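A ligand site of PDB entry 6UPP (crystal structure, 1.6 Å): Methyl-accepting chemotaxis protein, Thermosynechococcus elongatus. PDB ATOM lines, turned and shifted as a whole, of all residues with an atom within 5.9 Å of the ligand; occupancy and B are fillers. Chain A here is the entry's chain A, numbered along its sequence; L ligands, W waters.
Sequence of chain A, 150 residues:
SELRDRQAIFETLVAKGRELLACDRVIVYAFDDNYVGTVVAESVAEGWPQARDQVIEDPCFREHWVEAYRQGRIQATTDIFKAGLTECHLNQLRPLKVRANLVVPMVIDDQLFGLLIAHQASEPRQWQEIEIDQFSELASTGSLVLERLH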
ATOM      1  N   ILE A  27     -10.809 -28.734  16.560  1.00  0.00           N
ATOM      2  CA  ILE A  27     -10.502 -29.420  15.308  1.00  0.00           C
ATOM      3  C   ILE A  27      -9.000 -29.528  15.135  1.00  0.00           C
ATOM      4  O   ILE A  27      -8.222 -28.748  15.701  1.00  0.00           O
ATOM      5  CB  ILE A  27     -11.090 -28.699  14.067  1.00  0.00           C
ATOM      6  CG1 ILE A  27     -10.562 -27.279  14.029  1.00  0.00           C
ATOM      7  CG2 ILE A  27     -12.631 -28.737  14.094  1.00  0.00           C
ATOM      8  CD1 ILE A  27     -10.950 -26.507  12.727  1.00  0.00           C
ATOM      9  N   TYR A  29      -6.623 -29.194  11.894  1.00  0.00           N
ATOM     10  CA  TYR A  29      -6.634 -28.558  10.577  1.00  0.00           C
ATOM     11  C   TYR A  29      -5.262 -28.856   9.968  1.00  0.00           C
ATOM     12  O   TYR A  29      -4.252 -28.318  10.423  1.00  0.00           O
ATOM     13  CB  TYR A  29      -6.921 -27.069  10.763  1.00  0.00           C
ATOM     14  CG  TYR A  29      -6.934 -26.195   9.539  1.00  0.00           C
ATOM     15  CD1 TYR A  29      -8.008 -26.173   8.674  1.00  0.00           C
ATOM     16  CD2 TYR A  29      -5.904 -25.336   9.304  1.00  0.00           C
ATOM     17  CE1 TYR A  29      -8.015 -25.338   7.560  1.00  0.00           C
ATOM     18  CE2 TYR A  29      -5.907 -24.484   8.214  1.00  0.00           C
ATOM     19  CZ  TYR A  29      -6.969 -24.473   7.363  1.00  0.00           C
ATOM     20  OH  TYR A  29      -6.977 -23.652   6.247  1.00  0.00           O
ATOM     21  N   VAL A  39     -10.014 -29.985   7.557  1.00  0.00           N
ATOM     22  CA  VAL A  39     -10.467 -30.326   8.903  1.00  0.00           C
ATOM     23  C   VAL A  39     -10.541 -31.838   8.958  1.00  0.00           C
ATOM     24  O   VAL A  39     -11.473 -32.443   8.403  1.00  0.00           O
ATOM     25  CB  VAL A  39     -11.812 -29.686   9.240  1.00  0.00           C
ATOM     26  CG1 VAL A  39     -12.200 -30.014  10.683  1.00  0.00           C
ATOM     27  CG2 VAL A  39     -11.763 -28.189   9.017  1.00  0.00           C
ATOM     28  N   ILE A  56     -10.514 -25.960   3.499  1.00  0.00           N
ATOM     29  CA  ILE A  56     -10.576 -24.514   3.607  1.00  0.00           C
ATOM     30  C   ILE A  56      -9.237 -23.954   3.196  1.00  0.00           C
ATOM     31  O   ILE A  56      -8.240 -24.109   3.912  1.00  0.00           O
ATOM     32  CB  ILE A  56     -10.934 -24.059   5.042  1.00  0.00           C
ATOM     33  CG1 ILE A  56     -12.257 -24.676   5.479  1.00  0.00           C
ATOM     34  CG2 ILE A  56     -10.955 -22.532   5.106  1.00  0.00           C
ATOM     35  CD1 ILE A  56     -12.549 -24.499   6.941  1.00  0.00           C
ATOM     36  N   GLU A  57      -9.206 -23.257   2.061  1.00  0.00           N
ATOM     37  CA  GLU A  57      -7.982 -22.644   1.587  1.00  0.00           C
ATOM     38  C   GLU A  57      -7.917 -21.209   2.092  1.00  0.00           C
ATOM     39  O   GLU A  57      -8.748 -20.373   1.742  1.00  0.00           O
ATOM     40  CB  GLU A  57      -7.884 -22.651   0.062  1.00  0.00           C
ATOM     41  CG  GLU A  57      -6.717 -21.760  -0.398  1.00  0.00           C
ATOM     42  CD  GLU A  57      -6.380 -21.927  -1.865  1.00  0.00           C
ATOM     43  OE1 GLU A  57      -7.249 -22.394  -2.616  1.00  0.00           O
ATOM     44  OE2 GLU A  57      -5.251 -21.582  -2.256  1.00  0.00           O
ATOM     45  N   ASP A  58      -6.914 -20.936   2.914  1.00  0.00           N
ATOM     46  CA  ASP A  58      -6.712 -19.586   3.444  1.00  0.00           C
ATOM     47  C   ASP A  58      -5.279 -19.191   3.149  1.00  0.00           C
ATOM     48  O   ASP A  58      -4.339 -19.749   3.763  1.00  0.00           O
ATOM     49  CB  ASP A  58      -7.000 -19.554   4.953  1.00  0.00           C
ATOM     50  CG  ASP A  58      -6.914 -18.154   5.530  1.00  0.00           C
ATOM     51  OD1 ASP A  58      -6.303 -17.279   4.897  1.00  0.00           O
ATOM     52  OD2 ASP A  58      -7.497 -17.934   6.603  1.00  0.00           O
ATOM     53  N   PRO A  59      -5.045 -18.256   2.232  1.00  0.00           N
ATOM     54  CA  PRO A  59      -3.659 -17.956   1.837  1.00  0.00           C
ATOM     55  C   PRO A  59      -2.819 -17.284   2.916  1.00  0.00           C
ATOM     56  O   PRO A  59      -1.600 -17.184   2.736  1.00  0.00           O
ATOM     57  CB  PRO A  59      -3.819 -17.022   0.619  1.00  0.00           C
ATOM     58  CG  PRO A  59      -5.286 -16.877   0.378  1.00  0.00           C
ATOM     59  CD  PRO A  59      -6.027 -17.376   1.568  1.00  0.00           C
ATOM     60  N   CYS A  60      -3.399 -16.802   4.018  1.00  0.00           N
ATOM     61  CA  CYS A  60      -2.560 -16.019   4.933  1.00  0.00           C
ATOM     62  C   CYS A  60      -1.453 -16.870   5.541  1.00  0.00           C
ATOM     63  O   CYS A  60      -0.380 -16.337   5.892  1.00  0.00           O
ATOM     64  CB  CYS A  60      -3.396 -15.350   6.002  1.00  0.00           C
ATOM     65  SG  CYS A  60      -3.963 -16.481   7.324  1.00  0.00           S
ATOM     66  N   PHE A  61      -1.686 -18.169   5.736  1.00  0.00           N
ATOM     67  CA  PHE A  61      -0.664 -19.017   6.346  1.00  0.00           C
ATOM     68  C   PHE A  61       0.577 -19.071   5.467  1.00  0.00           C
ATOM     69  O   PHE A  61       1.673 -18.682   5.890  1.00  0.00           O
ATOM     70  CB  PHE A  61      -1.228 -20.412   6.624  1.00  0.00           C
ATOM     71  CG  PHE A  61      -2.317 -20.388   7.632  1.00  0.00           C
ATOM     72  CD1 PHE A  61      -2.051 -20.096   8.945  1.00  0.00           C
ATOM     73  CD2 PHE A  61      -3.627 -20.636   7.248  1.00  0.00           C
ATOM     74  CE1 PHE A  61      -3.064 -20.040   9.875  1.00  0.00           C
ATOM     75  CE2 PHE A  61      -4.649 -20.571   8.172  1.00  0.00           C
ATOM     76  CZ  PHE A  61      -4.370 -20.279   9.480  1.00  0.00           C
ATOM     77  N   GLU A  63       1.417 -17.161   3.082  1.00  0.00           N
ATOM     78  CA  GLU A  63       1.937 -15.866   2.692  1.00  0.00           C
ATOM     79  C   GLU A  63       2.665 -15.176   3.831  1.00  0.00           C
ATOM     80  O   GLU A  63       3.564 -14.392   3.568  1.00  0.00           O
ATOM     81  CB  GLU A  63       0.811 -14.989   2.164  1.00  0.00           C
ATOM     82  CG  GLU A  63       0.326 -15.487   0.811  1.00  0.00           C
ATOM     83  CD  GLU A  63      -0.639 -14.556   0.129  1.00  0.00           C
ATOM     84  OE1 GLU A  63      -0.890 -13.457   0.672  1.00  0.00           O
ATOM     85  OE2 GLU A  63      -1.147 -14.928  -0.948  1.00  0.00           O
ATOM     86  N   HIS A  64       2.312 -15.471   5.080  1.00  0.00           N
ATOM     87  CA  HIS A  64       2.835 -14.691   6.211  1.00  0.00           C
ATOM     88  C   HIS A  64       3.326 -15.520   7.381  1.00  0.00           C
ATOM     89  O   HIS A  64       4.283 -15.095   8.055  1.00  0.00           O
ATOM     90  CB  HIS A  64       1.732 -13.727   6.734  1.00  0.00           C
ATOM     91  CG  HIS A  64       1.196 -12.799   5.701  1.00  0.00           C
ATOM     92  ND1 HIS A  64       2.003 -12.112   4.829  1.00  0.00           N
ATOM     93  CD2 HIS A  64      -0.077 -12.444   5.401  1.00  0.00           C
ATOM     94  CE1 HIS A  64       1.258 -11.380   4.017  1.00  0.00           C
ATOM     95  NE2 HIS A  64      -0.013 -11.569   4.343  1.00  0.00           N
ATOM     96  N   TRP A  65       2.700 -16.659   7.681  1.00  0.00           N
ATOM     97  CA  TRP A  65       2.790 -17.174   9.045  1.00  0.00           C
ATOM     98  C   TRP A  65       3.338 -18.571   9.232  1.00  0.00           C
ATOM     99  O   TRP A  65       3.517 -18.984  10.372  1.00  0.00           O
ATOM    100  CB  TRP A  65       1.410 -17.119   9.740  1.00  0.00           C
ATOM    101  CG  TRP A  65       0.792 -15.781   9.668  1.00  0.00           C
ATOM    102  CD1 TRP A  65      -0.403 -15.459   9.100  1.00  0.00           C
ATOM    103  CD2 TRP A  65       1.340 -14.549  10.177  1.00  0.00           C
ATOM    104  NE1 TRP A  65      -0.636 -14.110   9.215  1.00  0.00           N
ATOM    105  CE2 TRP A  65       0.419 -13.523   9.881  1.00  0.00           C
ATOM    106  CE3 TRP A  65       2.515 -14.215  10.853  1.00  0.00           C
ATOM    107  CZ2 TRP A  65       0.633 -12.204  10.225  1.00  0.00           C
ATOM    108  CZ3 TRP A  65       2.730 -12.896  11.197  1.00  0.00           C
ATOM    109  CH2 TRP A  65       1.794 -11.903  10.889  1.00  0.00           C
ATOM    110  N   TYR A  69       4.448 -19.979  12.945  1.00  0.00           N
ATOM    111  CA  TYR A  69       3.784 -21.087  13.629  1.00  0.00           C
ATOM    112  C   TYR A  69       4.755 -22.223  13.949  1.00  0.00           C
ATOM    113  O   TYR A  69       4.680 -22.826  15.022  1.00  0.00           O
ATOM    114  CB  TYR A  69       2.580 -21.575  12.812  1.00  0.00           C
ATOM    115  CG  TYR A  69       1.343 -20.762  13.107  1.00  0.00           C
ATOM    116  CD1 TYR A  69       0.657 -20.890  14.328  1.00  0.00           C
ATOM    117  CD2 TYR A  69       0.862 -19.851  12.191  1.00  0.00           C
ATOM    118  CE1 TYR A  69      -0.479 -20.150  14.600  1.00  0.00           C
ATOM    119  CE2 TYR A  69      -0.283 -19.102  12.457  1.00  0.00           C
ATOM    120  CZ  TYR A  69      -0.935 -19.254  13.670  1.00  0.00           C
ATOM    121  OH  TYR A  69      -2.057 -18.491  13.919  1.00  0.00           O
ATOM    122  N   ARG A  73       4.243 -19.573  17.340  1.00  0.00           N
ATOM    123  CA  ARG A  73       3.139 -18.623  17.256  1.00  0.00           C
ATOM    124  C   ARG A  73       1.803 -19.286  17.579  1.00  0.00           C
ATOM    125  O   ARG A  73       1.566 -20.454  17.253  1.00  0.00           O
ATOM    126  CB  ARG A  73       3.070 -18.037  15.843  1.00  0.00           C
ATOM    127  CG  ARG A  73       2.072 -16.874  15.693  1.00  0.00           C
ATOM    128  CD  ARG A  73       1.950 -16.523  14.254  1.00  0.00           C
ATOM    129  NE  ARG A  73       1.033 -15.426  13.959  1.00  0.00           N
ATOM    130  CZ  ARG A  73       1.327 -14.146  14.076  1.00  0.00           C
ATOM    131  NH1 ARG A  73       2.514 -13.774  14.590  1.00  0.00           N
ATOM    132  NH2 ARG A  73       0.451 -13.231  13.717  1.00  0.00           N
ATOM    133  N   ILE A  74       0.911 -18.503  18.189  1.00  0.00           N
ATOM    134  CA  ILE A  74      -0.479 -18.871  18.362  1.00  0.00           C
ATOM    135  C   ILE A  74      -1.341 -17.756  17.774  1.00  0.00           C
ATOM    136  O   ILE A  74      -0.851 -16.683  17.395  1.00  0.00           O
ATOM    137  CB  ILE A  74      -0.839 -19.114  19.844  1.00  0.00           C
ATOM    138  CG1 ILE A  74      -0.788 -17.787  20.640  1.00  0.00           C
ATOM    139  CG2 ILE A  74       0.088 -20.149  20.432  1.00  0.00           C
ATOM    140  CD1 ILE A  74      -1.377 -17.880  22.070  1.00  0.00           C
ATOM    141  N   GLN A  75      -2.644 -18.015  17.736  1.00  0.00           N
ATOM    142  CA  GLN A  75      -3.624 -16.952  17.570  1.00  0.00           C
ATOM    143  C   GLN A  75      -4.628 -17.114  18.694  1.00  0.00           C
ATOM    144  O   GLN A  75      -5.257 -18.165  18.793  1.00  0.00           O
ATOM    145  CB  GLN A  75      -4.365 -16.996  16.226  1.00  0.00           C
ATOM    146  CG  GLN A  75      -5.529 -16.001  16.177  1.00  0.00           C
ATOM    147  CD  GLN A  75      -5.127 -14.568  15.819  1.00  0.00           C
ATOM    148  OE1 GLN A  75      -4.733 -14.304  14.690  1.00  0.00           O
ATOM    149  NE2 GLN A  75      -5.246 -13.644  16.790  1.00  0.00           N
ATOM    150  N   LEU A  85     -10.934  -8.022  10.729  1.00  0.00           N
ATOM    151  CA  LEU A  85     -10.833  -9.058   9.710  1.00  0.00           C
ATOM    152  C   LEU A  85     -11.627  -8.667   8.476  1.00  0.00           C
ATOM    153  O   LEU A  85     -12.618  -7.927   8.545  1.00  0.00           O
ATOM    154  CB  LEU A  85     -11.331 -10.397  10.269  1.00  0.00           C
ATOM    155  CG  LEU A  85     -10.572 -10.900  11.506  1.00  0.00           C
ATOM    156  CD1 LEU A  85     -11.346 -12.017  12.200  1.00  0.00           C
ATOM    157  CD2 LEU A  85      -9.166 -11.370  11.146  1.00  0.00           C
ATOM    158  N   THR A  86     -11.168  -9.149   7.324  1.00  0.00           N
ATOM    159  CA  THR A  86     -11.810  -8.877   6.047  1.00  0.00           C
ATOM    160  C   THR A  86     -13.041  -9.750   5.878  1.00  0.00           C
ATOM    161  O   THR A  86     -13.247 -10.740   6.575  1.00  0.00           O
ATOM    162  CB  THR A  86     -10.829  -9.133   4.904  1.00  0.00           C
ATOM    163  OG1 THR A  86     -10.499 -10.527   4.861  1.00  0.00           O
ATOM    164  CG2 THR A  86      -9.575  -8.339   5.102  1.00  0.00           C
ATOM    165  N   CYS A  88     -13.539 -11.697   3.469  1.00  0.00           N
ATOM    166  CA  CYS A  88     -13.157 -13.026   3.012  1.00  0.00           C
ATOM    167  C   CYS A  88     -12.881 -13.942   4.209  1.00  0.00           C
ATOM    168  O   CYS A  88     -13.362 -15.080   4.252  1.00  0.00           O
ATOM    169  CB  CYS A  88     -11.942 -12.956   2.091  1.00  0.00           C
ATOM    170  SG  CYS A  88     -11.467 -14.548   1.357  1.00  0.00           S
ATOM    171  N   HIS A  89     -12.194 -13.436   5.217  1.00  0.00           N
ATOM    172  CA  HIS A  89     -11.951 -14.220   6.432  1.00  0.00           C
ATOM    173  C   HIS A  89     -13.260 -14.523   7.157  1.00  0.00           C
ATOM    174  O   HIS A  89     -13.548 -15.675   7.514  1.00  0.00           O
ATOM    175  CB  HIS A  89     -10.978 -13.456   7.321  1.00  0.00           C
ATOM    176  CG  HIS A  89     -10.459 -14.243   8.478  1.00  0.00           C
ATOM    177  ND1 HIS A  89      -9.112 -14.385   8.746  1.00  0.00           N
ATOM    178  CD2 HIS A  89     -11.110 -14.909   9.466  1.00  0.00           C
ATOM    179  CE1 HIS A  89      -8.958 -15.118   9.832  1.00  0.00           C
ATOM    180  NE2 HIS A  89     -10.148 -15.452  10.293  1.00  0.00           N
ATOM    181  N   GLN A  92     -15.322 -17.263   5.478  1.00  0.00           N
ATOM    182  CA  GLN A  92     -14.870 -18.635   5.577  1.00  0.00           C
ATOM    183  C   GLN A  92     -15.228 -19.248   6.928  1.00  0.00           C
ATOM    184  O   GLN A  92     -15.392 -20.467   7.023  1.00  0.00           O
ATOM    185  CB  GLN A  92     -13.369 -18.725   5.288  1.00  0.00           C
ATOM    186  CG  GLN A  92     -12.438 -18.427   6.429  1.00  0.00           C
ATOM    187  CD  GLN A  92     -10.959 -18.371   6.014  1.00  0.00           C
ATOM    188  OE1 GLN A  92     -10.588 -18.831   4.924  1.00  0.00           O
ATOM    189  NE2 GLN A  92     -10.120 -17.812   6.883  1.00  0.00           N
ATOM    190  N   LEU A  93     -15.404 -18.413   7.959  1.00  0.00           N
ATOM    191  CA  LEU A  93     -15.794 -18.874   9.288  1.00  0.00           C
ATOM    192  C   LEU A  93     -17.307 -18.953   9.461  1.00  0.00           C
ATOM    193  O   LEU A  93     -17.790 -19.722  10.293  1.00  0.00           O
ATOM    194  CB  LEU A  93     -15.221 -17.939  10.354  1.00  0.00           C
ATOM    195  CG  LEU A  93     -13.691 -17.843  10.386  1.00  0.00           C
ATOM    196  CD1 LEU A  93     -13.205 -16.945  11.523  1.00  0.00           C
ATOM    197  CD2 LEU A  93     -13.059 -19.221  10.477  1.00  0.00           C
ATOM    198  N   LEU A  96     -19.250 -22.204   9.893  1.00  0.00           N
ATOM    199  CA  LEU A  96     -18.853 -23.006  11.052  1.00  0.00           C
ATOM    200  C   LEU A  96     -19.431 -22.450  12.334  1.00  0.00           C
ATOM    201  O   LEU A  96     -19.807 -23.220  13.221  1.00  0.00           O
ATOM    202  CB  LEU A  96     -17.323 -23.044  11.157  1.00  0.00           C
ATOM    203  CG  LEU A  96     -16.615 -23.648   9.955  1.00  0.00           C
ATOM    204  CD1 LEU A  96     -15.133 -23.821  10.272  1.00  0.00           C
ATOM    205  CD2 LEU A  96     -17.225 -24.964   9.565  1.00  0.00           C
ATOM    206  N   VAL A  98     -17.999 -19.180  14.421  1.00  0.00           N
ATOM    207  CA  VAL A  98     -16.846 -18.860  15.246  1.00  0.00           C
ATOM    208  C   VAL A  98     -17.013 -17.457  15.806  1.00  0.00           C
ATOM    209  O   VAL A  98     -17.099 -16.493  15.036  1.00  0.00           O
ATOM    210  CB  VAL A  98     -15.515 -18.932  14.458  1.00  0.00           C
ATOM    211  CG1 VAL A  98     -14.320 -18.691  15.393  1.00  0.00           C
ATOM    212  CG2 VAL A  98     -15.379 -20.239  13.721  1.00  0.00           C
ATOM    213  N   ASN A 101     -11.552 -17.662  18.944  1.00  0.00           N
ATOM    214  CA  ASN A 101     -10.784 -18.854  18.566  1.00  0.00           C
ATOM    215  C   ASN A 101      -9.375 -18.820  19.141  1.00  0.00           C
ATOM    216  O   ASN A 101      -8.835 -17.766  19.508  1.00  0.00           O
ATOM    217  CB  ASN A 101     -10.810 -19.115  17.052  1.00  0.00           C
ATOM    218  CG  ASN A 101     -10.192 -18.028  16.207  1.00  0.00           C
ATOM    219  OD1 ASN A 101      -9.842 -16.951  16.666  1.00  0.00           O
ATOM    220  ND2 ASN A 101     -10.037 -18.339  14.927  1.00  0.00           N
ATOM    221  N   VAL A 103      -5.711 -20.875  18.310  1.00  0.00           N
ATOM    222  CA  VAL A 103      -5.007 -21.613  17.281  1.00  0.00           C
ATOM    223  C   VAL A 103      -3.603 -21.894  17.794  1.00  0.00           C
ATOM    224  O   VAL A 103      -2.844 -20.968  18.078  1.00  0.00           O
ATOM    225  CB  VAL A 103      -4.976 -20.791  15.984  1.00  0.00           C
ATOM    226  CG1 VAL A 103      -4.200 -21.497  14.921  1.00  0.00           C
ATOM    227  CG2 VAL A 103      -6.403 -20.428  15.518  1.00  0.00           C
ATOM    228  N   ILE A 117      -7.173 -26.205  16.764  1.00  0.00           N
ATOM    229  CA  ILE A 117      -7.967 -24.985  16.839  1.00  0.00           C
ATOM    230  C   ILE A 117      -9.194 -25.224  17.698  1.00  0.00           C
ATOM    231  O   ILE A 117      -9.908 -26.221  17.513  1.00  0.00           O
ATOM    232  CB  ILE A 117      -8.381 -24.497  15.437  1.00  0.00           C
ATOM    233  CG1 ILE A 117      -7.131 -24.316  14.569  1.00  0.00           C
ATOM    234  CG2 ILE A 117      -9.222 -23.213  15.556  1.00  0.00           C
ATOM    235  CD1 ILE A 117      -7.405 -23.904  13.127  1.00  0.00           C
ATOM    236  N   ALA A 118      -9.427 -24.304  18.637  1.00  0.00           N
ATOM    237  CA  ALA A 118     -10.619 -24.270  19.471  1.00  0.00           C
ATOM    238  C   ALA A 118     -11.495 -23.091  19.077  1.00  0.00           C
ATOM    239  O   ALA A 118     -10.987 -21.989  18.829  1.00  0.00           O
ATOM    240  CB  ALA A 118     -10.249 -24.159  20.946  1.00  0.00           C
ATOM    241  N   HIS A 119     -12.810 -23.326  19.082  1.00  0.00           N
ATOM    242  CA  HIS A 119     -13.807 -22.320  18.791  1.00  0.00           C
ATOM    243  C   HIS A 119     -14.788 -22.196  19.952  1.00  0.00           C
ATOM    244  O   HIS A 119     -15.241 -23.207  20.503  1.00  0.00           O
ATOM    245  CB  HIS A 119     -14.633 -22.672  17.540  1.00  0.00           C
ATOM    246  CG  HIS A 119     -13.861 -22.682  16.268  1.00  0.00           C
ATOM    247  ND1 HIS A 119     -14.273 -23.424  15.176  1.00  0.00           N
ATOM    248  CD2 HIS A 119     -12.742 -22.035  15.888  1.00  0.00           C
ATOM    249  CE1 HIS A 119     -13.422 -23.226  14.177  1.00  0.00           C
ATOM    250  NE2 HIS A 119     -12.477 -22.399  14.586  1.00  0.00           N
HETATM  251  C1  LIG L   1     -10.067 -16.557   2.336  1.00  0.00           C
HETATM  252  C2  LIG L   1     -10.122 -15.013   2.319  1.00  0.00           C
HETATM  253  C3  LIG L   1      -8.688 -14.374   2.402  1.00  0.00           C
HETATM  254  C4  LIG L   1      -7.849 -14.337   1.375  1.00  0.00           C
HETATM  255  C5  LIG L   1      -8.040 -14.968   0.008  1.00  0.00           C
HETATM  256  C6  LIG L   1      -6.675 -13.607   1.868  1.00  0.00           C
HETATM  257  O1  LIG L   1      -5.704 -13.406   1.173  1.00  0.00           O
HETATM  258  N1  LIG L   1      -6.788 -13.202   3.160  1.00  0.00           N
HETATM  259  C7  LIG L   1      -8.128 -13.602   3.604  1.00  0.00           C
HETATM  260  C8  LIG L   1      -8.212 -14.454   4.850  1.00  0.00           C
HETATM  261  C9  LIG L   1      -7.323 -14.079   5.992  1.00  0.00           C
HETATM  262  C10 LIG L   1      -7.141 -12.910   6.681  1.00  0.00           C
HETATM  263  C11 LIG L   1      -7.805 -11.583   6.428  1.00  0.00           C
HETATM  264  C12 LIG L   1      -6.190 -13.155   7.683  1.00  0.00           C
HETATM  265  C13 LIG L   1      -5.837 -14.513   7.583  1.00  0.00           C
HETATM  266  C14 LIG L   1      -4.829 -15.369   8.395  1.00  0.00           C
HETATM  267  C15 LIG L   1      -5.564 -16.359   9.352  1.00  0.00           C
HETATM  268  C16 LIG L   1      -5.418 -16.441  10.758  1.00  0.00           C
HETATM  269  C17 LIG L   1      -4.536 -15.529  11.594  1.00  0.00           C
HETATM  270  C18 LIG L   1      -3.086 -15.952  11.500  1.00  0.00           C
HETATM  271  C19 LIG L   1      -2.187 -15.246  12.495  1.00  0.00           C
HETATM  272  O2  LIG L   1      -1.530 -15.988  13.352  1.00  0.00           O
HETATM  273  O3  LIG L   1      -2.025 -14.032  12.488  1.00  0.00           O
HETATM  274  C20 LIG L   1      -6.235 -17.479  11.157  1.00  0.00           C
HETATM  275  C21 LIG L   1      -6.884 -18.008   9.985  1.00  0.00           C
HETATM  276  N2  LIG L   1      -6.444 -17.283   8.963  1.00  0.00           N
HETATM  277  C22 LIG L   1      -7.826 -19.106   9.653  1.00  0.00           C
HETATM  278  C23 LIG L   1      -8.622 -19.876  10.492  1.00  0.00           C
HETATM  279  N3  LIG L   1      -9.076 -19.639  11.779  1.00  0.00           N
HETATM  280  C24 LIG L   1      -9.822 -20.698  12.166  1.00  0.00           C
HETATM  281  O4  LIG L   1     -10.387 -20.832  13.237  1.00  0.00           O
HETATM  282  C25 LIG L   1      -9.877 -21.631  11.110  1.00  0.00           C
HETATM  283  C26 LIG L   1      -9.132 -21.138  10.094  1.00  0.00           C
HETATM  284  C27 LIG L   1      -8.900 -21.809   8.754  1.00  0.00           C
HETATM  285  C28 LIG L   1     -10.603 -22.965  11.159  1.00  0.00           C
HETATM  286  C29 LIG L   1     -12.058 -22.782  10.756  1.00  0.00           C
HETATM  287  C30 LIG L   1      -6.389 -17.934  12.589  1.00  0.00           C
HETATM  288  N4  LIG L   1      -6.538 -15.041   6.543  1.00  0.00           N
HETATM  289  C31 LIG L   1      -5.631 -12.198   8.714  1.00  0.00           C
HETATM  290  C32 LIG L   1      -4.599 -11.216   8.140  1.00  0.00           C
HETATM  291  C33 LIG L   1      -3.354 -11.941   7.684  1.00  0.00           C
HETATM  292  O5  LIG L   1      -2.763 -12.686   8.424  1.00  0.00           O
HETATM  293  O6  LIG L   1      -2.931 -11.740   6.432  1.00  0.00           O
HETATM  294  O   HOH W   1      -3.014 -12.088  11.141  1.00  0.00           O
HETATM  295  O   HOH W   2      -4.310 -12.363   4.188  1.00  0.00           O
HETATM  296  O   HOH W   3      -8.821 -10.766   2.833  1.00  0.00           O
HETATM  297  O   HOH W   4      -5.244 -12.980  -1.434  1.00  0.00           O
HETATM  298  O   HOH W   5      -3.292  -8.675   5.747  1.00  0.00           O
HETATM  299  O   HOH W   6      -9.473 -16.387  12.762  1.00  0.00           O
HETATM  300  O   HOH W   7      -6.053  -9.971   3.458  1.00  0.00           O
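A carbon (C2) of the ligand is covalently linked to the side-chain sulfur of Cys 88 (1.7 Å).
The side-chain sulfur (SG) of Cys 60 is bonded to a carbon (C14) of the ligand (1.8 Å).
An oxygen (O2) of the ligand lies within hydrogen-bond range of the side-chain hydroxyl of Tyr 69 (2.6 Å).
The side-chain carboxylate (OD2) of Asp 58 lies within hydrogen-bond range of a nitrogen (N2) of the ligand (2.7 Å).
The indole nitrogen (NE1) of Trp 65 lies within hydrogen-bond range of an oxygen (O5) of the ligand.
NE of Arg 73 is in salt-bridge range of O2 of the ligand, 2.7 Å away.
NE2 of His 119 sits at hydrogen-bond distance from O4 of the ligand (2.9 Å).
The side-chain amide nitrogen (ND2) of Asn 101 is in hydrogen-bond range of an oxygen (O4) of the ligand, at 3.0 Å.
A ring nitrogen (ND1) of His 89 lies close to a nitrogen (N4) of the ligand (3.5 Å).
N of Cys 60 is in hydrogen-bond range of OD1 of Asp 58 (3.1 Å).
The side-chain carboxylate (OD2) of Asp 58 lies within hydrogen-bond range of the side-chain amide nitrogen (NE2) of Gln 92 (2.6 Å).
OG1 of Thr 86 is in hydrogen-bond range of N of His 89 (3.4 Å).
N of Val 103 lies within hydrogen-bond range of O of Gln 75, at 2.8 Å.
O of Ile 117 sits at hydrogen-bond distance from N of Ile 27, 2.8 Å away.
O of Ile 56 lies within hydrogen-bond range of OH of Tyr 29, at 2.7 Å.
Merely in contact with the ligand: Ile 27 (3.9 Å), Tyr 29 (3.6 Å), Pro 59 (3.4 Å), Phe 61 (3.4 Å), His 64 (3.1 Å), Gln 75 (3.3 Å), Thr 86 (3.3 Å), Gln 92 (3.5 Å), Leu 93 (3.7 Å), Leu 96 (3.3 Å), Val 103 (3.8 Å) and Ile 117 (3.5 Å).
Hydrophobic or aromatic side chains within 4 Å of the ligand: Ile 27, Tyr 29, Pro 59, Phe 61, His 64, Trp 65, Tyr 69, His 89, Leu 93, Leu 96, Val 103, Ile 117 and His 119.
Of the 29 residues printed, 21 come within 4 Å of the ligand.
The nearest printed residue that does not touch the ligand is Glu 57 (4.1 Å).
Water W3 lies within hydrogen-bond range of the side-chain hydroxyl (OG1) of Thr 86 (2.6 Å) and a nitrogen (N1) of the ligand (3.2 Å).
Water W6 lies within hydrogen-bond range of NE2 of His 89 (2.7 Å), ND2 of Asn 101 (3.0 Å) and N3 of the ligand (3.4 Å).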
